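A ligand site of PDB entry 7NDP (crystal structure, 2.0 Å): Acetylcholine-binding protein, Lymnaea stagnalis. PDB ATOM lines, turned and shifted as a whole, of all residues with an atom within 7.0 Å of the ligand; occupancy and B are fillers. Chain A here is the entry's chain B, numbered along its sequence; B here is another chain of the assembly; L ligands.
OH of Tyr 108 sits at hydrogen-bond distance from N1 of the ligand (2.7 Å). The backbone carbonyl oxygen (O) of Trp 162 lies within hydrogen-bond range of a nitrogen (N1) of the ligand (3.1 Å).
The side-chain hydroxyl of Tyr 108 sits at hydrogen-bond distance from the backbone carbonyl oxygen of Ser 161, 3.3 Å away. NE1 of Trp 162 lies within hydrogen-bond range of O of Met 133 of chain B (2.8 Å). SG of Cys 206 is disulfide-bonded to SG of Cys 207 (2.1 Å). O of Lys 53 of chain B lies within hydrogen-bond range of N of Trp 72 of chain B (2.8 Å).
SG of Cys 206 sits close to O1 of the ligand (3.8 Å). SG of Cys 207 lies close to O1 of the ligand (3.5 Å). Residues that only touch the ligand: Tyr 204 (3.9 Å), Tyr 211 (3.3 Å), Lys 53 of chain B (3.6 Å), Trp 72 of chain B (3.6 Å), Gln 74 of chain B (3.99 Å), Met 133 of chain B (3.0 Å) and Tyr 183 of chain B (3.8 Å). Hydrophobic or aromatic side chains that line the ligand: Tyr 108, Trp 162, Tyr 204, Tyr 211, Trp 72 of chain B, Met 133 of chain B and Tyr 183 of chain B.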
ATOM      1  N   TYR A 108     -25.620  -0.792  14.292  1.00  0.00           N
ATOM      2  CA  TYR A 108     -26.686  -1.053  15.289  1.00  0.00           C
ATOM      3  C   TYR A 108     -27.362  -2.412  15.018  1.00  0.00           C
ATOM      4  O   TYR A 108     -27.837  -3.028  15.972  1.00  0.00           O
ATOM      5  CB  TYR A 108     -27.696   0.097  15.361  1.00  0.00           C
ATOM      6  CG  TYR A 108     -27.152   1.241  16.180  1.00  0.00           C
ATOM      7  CD1 TYR A 108     -26.084   1.996  15.723  1.00  0.00           C
ATOM      8  CD2 TYR A 108     -27.626   1.504  17.449  1.00  0.00           C
ATOM      9  CE1 TYR A 108     -25.542   3.019  16.484  1.00  0.00           C
ATOM     10  CE2 TYR A 108     -27.078   2.510  18.235  1.00  0.00           C
ATOM     11  CZ  TYR A 108     -26.033   3.282  17.754  1.00  0.00           C
ATOM     12  OH  TYR A 108     -25.440   4.275  18.491  1.00  0.00           O
ATOM     13  N   GLY A 160     -23.189   4.456  13.691  1.00  0.00           N
ATOM     14  CA  GLY A 160     -22.928   5.659  14.505  1.00  0.00           C
ATOM     15  C   GLY A 160     -21.873   5.412  15.562  1.00  0.00           C
ATOM     16  O   GLY A 160     -21.511   4.235  15.794  1.00  0.00           O
ATOM     17  N   SER A 161     -21.465   6.463  16.250  1.00  0.00           N
ATOM     18  CA  SER A 161     -20.615   6.380  17.461  1.00  0.00           C
ATOM     19  C   SER A 161     -21.396   5.603  18.520  1.00  0.00           C
ATOM     20  O   SER A 161     -22.573   5.933  18.757  1.00  0.00           O
ATOM     21  CB  SER A 161     -20.207   7.711  17.964  1.00  0.00           C
ATOM     22  OG  SER A 161     -19.519   7.554  19.199  1.00  0.00           O
ATOM     23  N   TRP A 162     -20.754   4.627  19.158  1.00  0.00           N
ATOM     24  CA  TRP A 162     -21.385   3.863  20.255  1.00  0.00           C
ATOM     25  C   TRP A 162     -21.506   4.732  21.521  1.00  0.00           C
ATOM     26  O   TRP A 162     -22.483   4.564  22.242  1.00  0.00           O
ATOM     27  CB  TRP A 162     -20.619   2.554  20.502  1.00  0.00           C
ATOM     28  CG  TRP A 162     -21.382   1.625  21.379  1.00  0.00           C
ATOM     29  CD1 TRP A 162     -21.048   1.182  22.626  1.00  0.00           C
ATOM     30  CD2 TRP A 162     -22.657   1.047  21.077  1.00  0.00           C
ATOM     31  NE1 TRP A 162     -22.047   0.399  23.137  1.00  0.00           N
ATOM     32  CE2 TRP A 162     -23.033   0.269  22.201  1.00  0.00           C
ATOM     33  CE3 TRP A 162     -23.540   1.128  19.996  1.00  0.00           C
ATOM     34  CZ2 TRP A 162     -24.229  -0.431  22.250  1.00  0.00           C
ATOM     35  CZ3 TRP A 162     -24.707   0.409  20.033  1.00  0.00           C
ATOM     36  CH2 TRP A 162     -25.054  -0.361  21.154  1.00  0.00           C
ATOM     37  N   THR A 163     -20.551   5.612  21.812  1.00  0.00           N
ATOM     38  CA  THR A 163     -20.535   6.314  23.119  1.00  0.00           C
ATOM     39  C   THR A 163     -20.511   7.842  22.999  1.00  0.00           C
ATOM     40  O   THR A 163     -20.621   8.475  24.048  1.00  0.00           O
ATOM     41  CB  THR A 163     -19.348   5.844  23.975  1.00  0.00           C
ATOM     42  OG1 THR A 163     -18.127   6.359  23.427  1.00  0.00           O
ATOM     43  CG2 THR A 163     -19.291   4.336  24.097  1.00  0.00           C
ATOM     44  N   HIS A 164     -20.294   8.411  21.814  1.00  0.00           N
ATOM     45  CA  HIS A 164     -20.178   9.889  21.665  1.00  0.00           C
ATOM     46  C   HIS A 164     -21.454  10.438  21.005  1.00  0.00           C
ATOM     47  O   HIS A 164     -21.782  10.015  19.878  1.00  0.00           O
ATOM     48  CB  HIS A 164     -18.934  10.256  20.862  1.00  0.00           C
ATOM     49  CG  HIS A 164     -17.639   9.915  21.508  1.00  0.00           C
ATOM     50  ND1 HIS A 164     -17.102  10.681  22.536  1.00  0.00           N
ATOM     51  CD2 HIS A 164     -16.741   8.952  21.241  1.00  0.00           C
ATOM     52  CE1 HIS A 164     -15.934  10.178  22.889  1.00  0.00           C
ATOM     53  NE2 HIS A 164     -15.685   9.119  22.112  1.00  0.00           N
ATOM     54  N   HIS A 165     -22.121  11.381  21.666  1.00  0.00           N
ATOM     55  CA  HIS A 165     -23.324  12.104  21.147  1.00  0.00           C
ATOM     56  C   HIS A 165     -22.884  13.225  20.193  1.00  0.00           C
ATOM     57  O   HIS A 165     -21.655  13.422  20.015  1.00  0.00           O
ATOM     58  CB  HIS A 165     -24.207  12.568  22.317  1.00  0.00           C
ATOM     59  CG  HIS A 165     -23.484  13.421  23.306  1.00  0.00           C
ATOM     60  ND1 HIS A 165     -22.998  14.673  22.974  1.00  0.00           N
ATOM     61  CD2 HIS A 165     -23.148  13.197  24.594  1.00  0.00           C
ATOM     62  CE1 HIS A 165     -22.387  15.173  24.025  1.00  0.00           C
ATOM     63  NE2 HIS A 165     -22.466  14.291  25.032  1.00  0.00           N
ATOM     64  N   TYR A 204     -32.837   9.103  22.063  1.00  0.00           N
ATOM     65  CA  TYR A 204     -33.438   7.917  22.708  1.00  0.00           C
ATOM     66  C   TYR A 204     -34.007   8.337  24.067  1.00  0.00           C
ATOM     67  O   TYR A 204     -33.550   9.351  24.609  1.00  0.00           O
ATOM     68  CB  TYR A 204     -32.385   6.811  22.800  1.00  0.00           C
ATOM     69  CG  TYR A 204     -31.845   6.386  21.457  1.00  0.00           C
ATOM     70  CD1 TYR A 204     -30.803   7.064  20.863  1.00  0.00           C
ATOM     71  CD2 TYR A 204     -32.392   5.301  20.786  1.00  0.00           C
ATOM     72  CE1 TYR A 204     -30.301   6.677  19.622  1.00  0.00           C
ATOM     73  CE2 TYR A 204     -31.907   4.901  19.540  1.00  0.00           C
ATOM     74  CZ  TYR A 204     -30.865   5.594  18.964  1.00  0.00           C
ATOM     75  OH  TYR A 204     -30.380   5.223  17.742  1.00  0.00           O
ATOM     76  N   SER A 205     -34.993   7.575  24.582  1.00  0.00           N
ATOM     77  CA  SER A 205     -35.692   7.831  25.878  1.00  0.00           C
ATOM     78  C   SER A 205     -34.679   7.879  27.035  1.00  0.00           C
ATOM     79  O   SER A 205     -34.813   8.794  27.871  1.00  0.00           O
ATOM     80  CB  SER A 205     -36.766   6.805  26.131  1.00  0.00           C
ATOM     81  OG  SER A 205     -37.571   6.622  24.985  1.00  0.00           O
ATOM     82  N   CYS A 206     -33.700   6.968  27.052  1.00  0.00           N
ATOM     83  CA  CYS A 206     -32.628   6.852  28.079  1.00  0.00           C
ATOM     84  C   CYS A 206     -31.952   8.203  28.373  1.00  0.00           C
ATOM     85  O   CYS A 206     -31.636   8.438  29.540  1.00  0.00           O
ATOM     86  CB  CYS A 206     -31.530   5.876  27.632  1.00  0.00           C
ATOM     87  SG  CYS A 206     -30.613   6.426  26.165  1.00  0.00           S
ATOM     88  N   CYS A 207     -31.730   9.023  27.346  1.00  0.00           N
ATOM     89  CA  CYS A 207     -30.579   9.959  27.272  1.00  0.00           C
ATOM     90  C   CYS A 207     -31.025  11.308  26.717  1.00  0.00           C
ATOM     91  O   CYS A 207     -31.757  11.362  25.724  1.00  0.00           O
ATOM     92  CB  CYS A 207     -29.484   9.345  26.396  1.00  0.00           C
ATOM     93  SG  CYS A 207     -29.072   7.632  26.834  1.00  0.00           S
ATOM     94  N   TYR A 211     -27.736  11.335  19.062  1.00  0.00           N
ATOM     95  CA  TYR A 211     -26.680  10.490  18.449  1.00  0.00           C
ATOM     96  C   TYR A 211     -26.867  10.476  16.941  1.00  0.00           C
ATOM     97  O   TYR A 211     -27.975  10.173  16.460  1.00  0.00           O
ATOM     98  CB  TYR A 211     -26.713   9.078  19.030  1.00  0.00           C
ATOM     99  CG  TYR A 211     -26.274   9.050  20.476  1.00  0.00           C
ATOM    100  CD1 TYR A 211     -27.197   9.323  21.472  1.00  0.00           C
ATOM    101  CD2 TYR A 211     -24.948   8.848  20.846  1.00  0.00           C
ATOM    102  CE1 TYR A 211     -26.840   9.307  22.810  1.00  0.00           C
ATOM    103  CE2 TYR A 211     -24.586   8.834  22.177  1.00  0.00           C
ATOM    104  CZ  TYR A 211     -25.520   9.073  23.164  1.00  0.00           C
ATOM    105  OH  TYR A 211     -25.158   9.081  24.477  1.00  0.00           O
ATOM    106  N   LYS B  53     -31.537  -5.087  27.257  1.00  0.00           N
ATOM    107  CA  LYS B  53     -32.423  -4.655  26.144  1.00  0.00           C
ATOM    108  C   LYS B  53     -32.249  -5.675  25.017  1.00  0.00           C
ATOM    109  O   LYS B  53     -31.156  -5.703  24.414  1.00  0.00           O
ATOM    110  CB  LYS B  53     -32.083  -3.248  25.645  1.00  0.00           C
ATOM    111  CG  LYS B  53     -31.675  -2.236  26.705  1.00  0.00           C
ATOM    112  CD  LYS B  53     -32.723  -1.898  27.735  1.00  0.00           C
ATOM    113  CE  LYS B  53     -32.177  -0.929  28.764  1.00  0.00           C
ATOM    114  NZ  LYS B  53     -33.006  -0.862  29.987  1.00  0.00           N
ATOM    115  N   TRP B  72     -28.330  -5.621  24.500  1.00  0.00           N
ATOM    116  CA  TRP B  72     -27.525  -4.528  25.080  1.00  0.00           C
ATOM    117  C   TRP B  72     -27.571  -4.691  26.587  1.00  0.00           C
ATOM    118  O   TRP B  72     -28.689  -4.725  27.137  1.00  0.00           O
ATOM    119  CB  TRP B  72     -28.039  -3.172  24.633  1.00  0.00           C
ATOM    120  CG  TRP B  72     -28.021  -3.001  23.147  1.00  0.00           C
ATOM    121  CD1 TRP B  72     -27.385  -3.786  22.223  1.00  0.00           C
ATOM    122  CD2 TRP B  72     -28.623  -1.938  22.415  1.00  0.00           C
ATOM    123  NE1 TRP B  72     -27.580  -3.284  20.970  1.00  0.00           N
ATOM    124  CE2 TRP B  72     -28.330  -2.145  21.060  1.00  0.00           C
ATOM    125  CE3 TRP B  72     -29.398  -0.834  22.785  1.00  0.00           C
ATOM    126  CZ2 TRP B  72     -28.782  -1.292  20.054  1.00  0.00           C
ATOM    127  CZ3 TRP B  72     -29.851   0.008  21.787  1.00  0.00           C
ATOM    128  CH2 TRP B  72     -29.545  -0.212  20.448  1.00  0.00           C
ATOM    129  N   GLN B  74     -27.101  -3.029  29.665  1.00  0.00           N
ATOM    130  CA  GLN B  74     -26.991  -1.709  30.334  1.00  0.00           C
ATOM    131  C   GLN B  74     -26.513  -1.921  31.768  1.00  0.00           C
ATOM    132  O   GLN B  74     -27.229  -2.587  32.541  1.00  0.00           O
ATOM    133  CB  GLN B  74     -28.313  -0.949  30.269  1.00  0.00           C
ATOM    134  CG  GLN B  74     -28.254   0.441  30.912  1.00  0.00           C
ATOM    135  CD  GLN B  74     -29.594   1.116  30.856  1.00  0.00           C
ATOM    136  OE1 GLN B  74     -30.095   1.327  29.752  1.00  0.00           O
ATOM    137  NE2 GLN B  74     -30.197   1.439  31.988  1.00  0.00           N
ATOM    138  N   LEU B 131     -21.283   4.263  33.008  1.00  0.00           N
ATOM    139  CA  LEU B 131     -22.274   3.530  32.175  1.00  0.00           C
ATOM    140  C   LEU B 131     -21.502   2.679  31.160  1.00  0.00           C
ATOM    141  O   LEU B 131     -20.724   3.251  30.373  1.00  0.00           O
ATOM    142  CB  LEU B 131     -23.206   4.524  31.461  1.00  0.00           C
ATOM    143  CG  LEU B 131     -23.475   5.824  32.219  1.00  0.00           C
ATOM    144  CD1 LEU B 131     -23.907   6.948  31.272  1.00  0.00           C
ATOM    145  CD2 LEU B 131     -24.522   5.629  33.304  1.00  0.00           C
ATOM    146  N   MET B 133     -22.430  -0.242  28.328  1.00  0.00           N
ATOM    147  CA  MET B 133     -23.528  -0.955  27.630  1.00  0.00           C
ATOM    148  C   MET B 133     -22.995  -1.631  26.373  1.00  0.00           C
ATOM    149  O   MET B 133     -23.158  -1.108  25.267  1.00  0.00           O
ATOM    150  CB  MET B 133     -24.680  -0.025  27.261  1.00  0.00           C
ATOM    151  CG  MET B 133     -25.953  -0.810  26.888  1.00  0.00           C
ATOM    152  SD  MET B 133     -27.398   0.201  26.539  1.00  0.00           S
ATOM    153  CE  MET B 133     -27.130   1.599  27.621  1.00  0.00           C
ATOM    154  N   GLU B 182     -38.425  -2.397  23.215  1.00  0.00           N
ATOM    155  CA  GLU B 182     -38.637  -1.249  22.296  1.00  0.00           C
ATOM    156  C   GLU B 182     -37.699  -1.336  21.082  1.00  0.00           C
ATOM    157  O   GLU B 182     -38.093  -0.857  20.023  1.00  0.00           O
ATOM    158  CB  GLU B 182     -38.387   0.060  23.050  1.00  0.00           C
ATOM    159  CG  GLU B 182     -38.396   1.280  22.151  1.00  0.00           C
ATOM    160  CD  GLU B 182     -38.505   2.653  22.807  1.00  0.00           C
ATOM    161  OE1 GLU B 182     -38.716   3.617  22.042  1.00  0.00           O
ATOM    162  OE2 GLU B 182     -38.397   2.767  24.049  1.00  0.00           O
ATOM    163  N   TYR B 183     -36.495  -1.893  21.235  1.00  0.00           N
ATOM    164  CA  TYR B 183     -35.432  -1.876  20.201  1.00  0.00           C
ATOM    165  C   TYR B 183     -35.236  -3.266  19.590  1.00  0.00           C
ATOM    166  O   TYR B 183     -34.263  -3.510  18.861  1.00  0.00           O
ATOM    167  CB  TYR B 183     -34.158  -1.299  20.811  1.00  0.00           C
ATOM    168  CG  TYR B 183     -34.379   0.097  21.329  1.00  0.00           C
ATOM    169  CD1 TYR B 183     -34.747   1.117  20.456  1.00  0.00           C
ATOM    170  CD2 TYR B 183     -34.325   0.388  22.684  1.00  0.00           C
ATOM    171  CE1 TYR B 183     -35.004   2.402  20.907  1.00  0.00           C
ATOM    172  CE2 TYR B 183     -34.582   1.675  23.149  1.00  0.00           C
ATOM    173  CZ  TYR B 183     -34.916   2.680  22.258  1.00  0.00           C
ATOM    174  OH  TYR B 183     -35.174   3.932  22.736  1.00  0.00           O
HETATM  175  O1  LIG L   1     -27.514   4.515  27.170  1.00  0.00           O
HETATM  176  C1  LIG L   1     -27.632   4.484  25.950  1.00  0.00           C
HETATM  177  C2  LIG L   1     -28.832   3.845  25.321  1.00  0.00           C
HETATM  178  C3  LIG L   1     -26.578   5.127  25.082  1.00  0.00           C
HETATM  179  C4  LIG L   1     -26.687   4.716  23.604  1.00  0.00           C
HETATM  180  C5  LIG L   1     -25.946   3.413  23.384  1.00  0.00           C
HETATM  181  C6  LIG L   1     -26.025   3.085  21.907  1.00  0.00           C
HETATM  182  N1  LIG L   1     -25.363   4.162  21.164  1.00  0.00           N
HETATM  183  C7  LIG L   1     -26.117   5.413  21.278  1.00  0.00           C
HETATM  184  C8  LIG L   1     -26.101   5.818  22.737  1.00  0.00           C
HETATM  185  O2  LIG L   1     -28.013   4.538  23.099  1.00  0.00           O
HETATM  186  C9  LIG L   1     -28.971   3.918  23.840  1.00  0.00           C
HETATM  187  C10 LIG L   1     -30.078   3.348  23.226  1.00  0.00           C
HETATM  188  C11 LIG L   1     -31.041   2.732  24.016  1.00  0.00           C
HETATM  189  C12 LIG L   1     -30.915   2.661  25.411  1.00  0.00           C
HETATM  190 BR1  LIG L   1     -32.258   1.801  26.430  1.00  0.00          BR
HETATM  191  C13 LIG L   1     -29.825   3.214  26.071  1.00  0.00           C
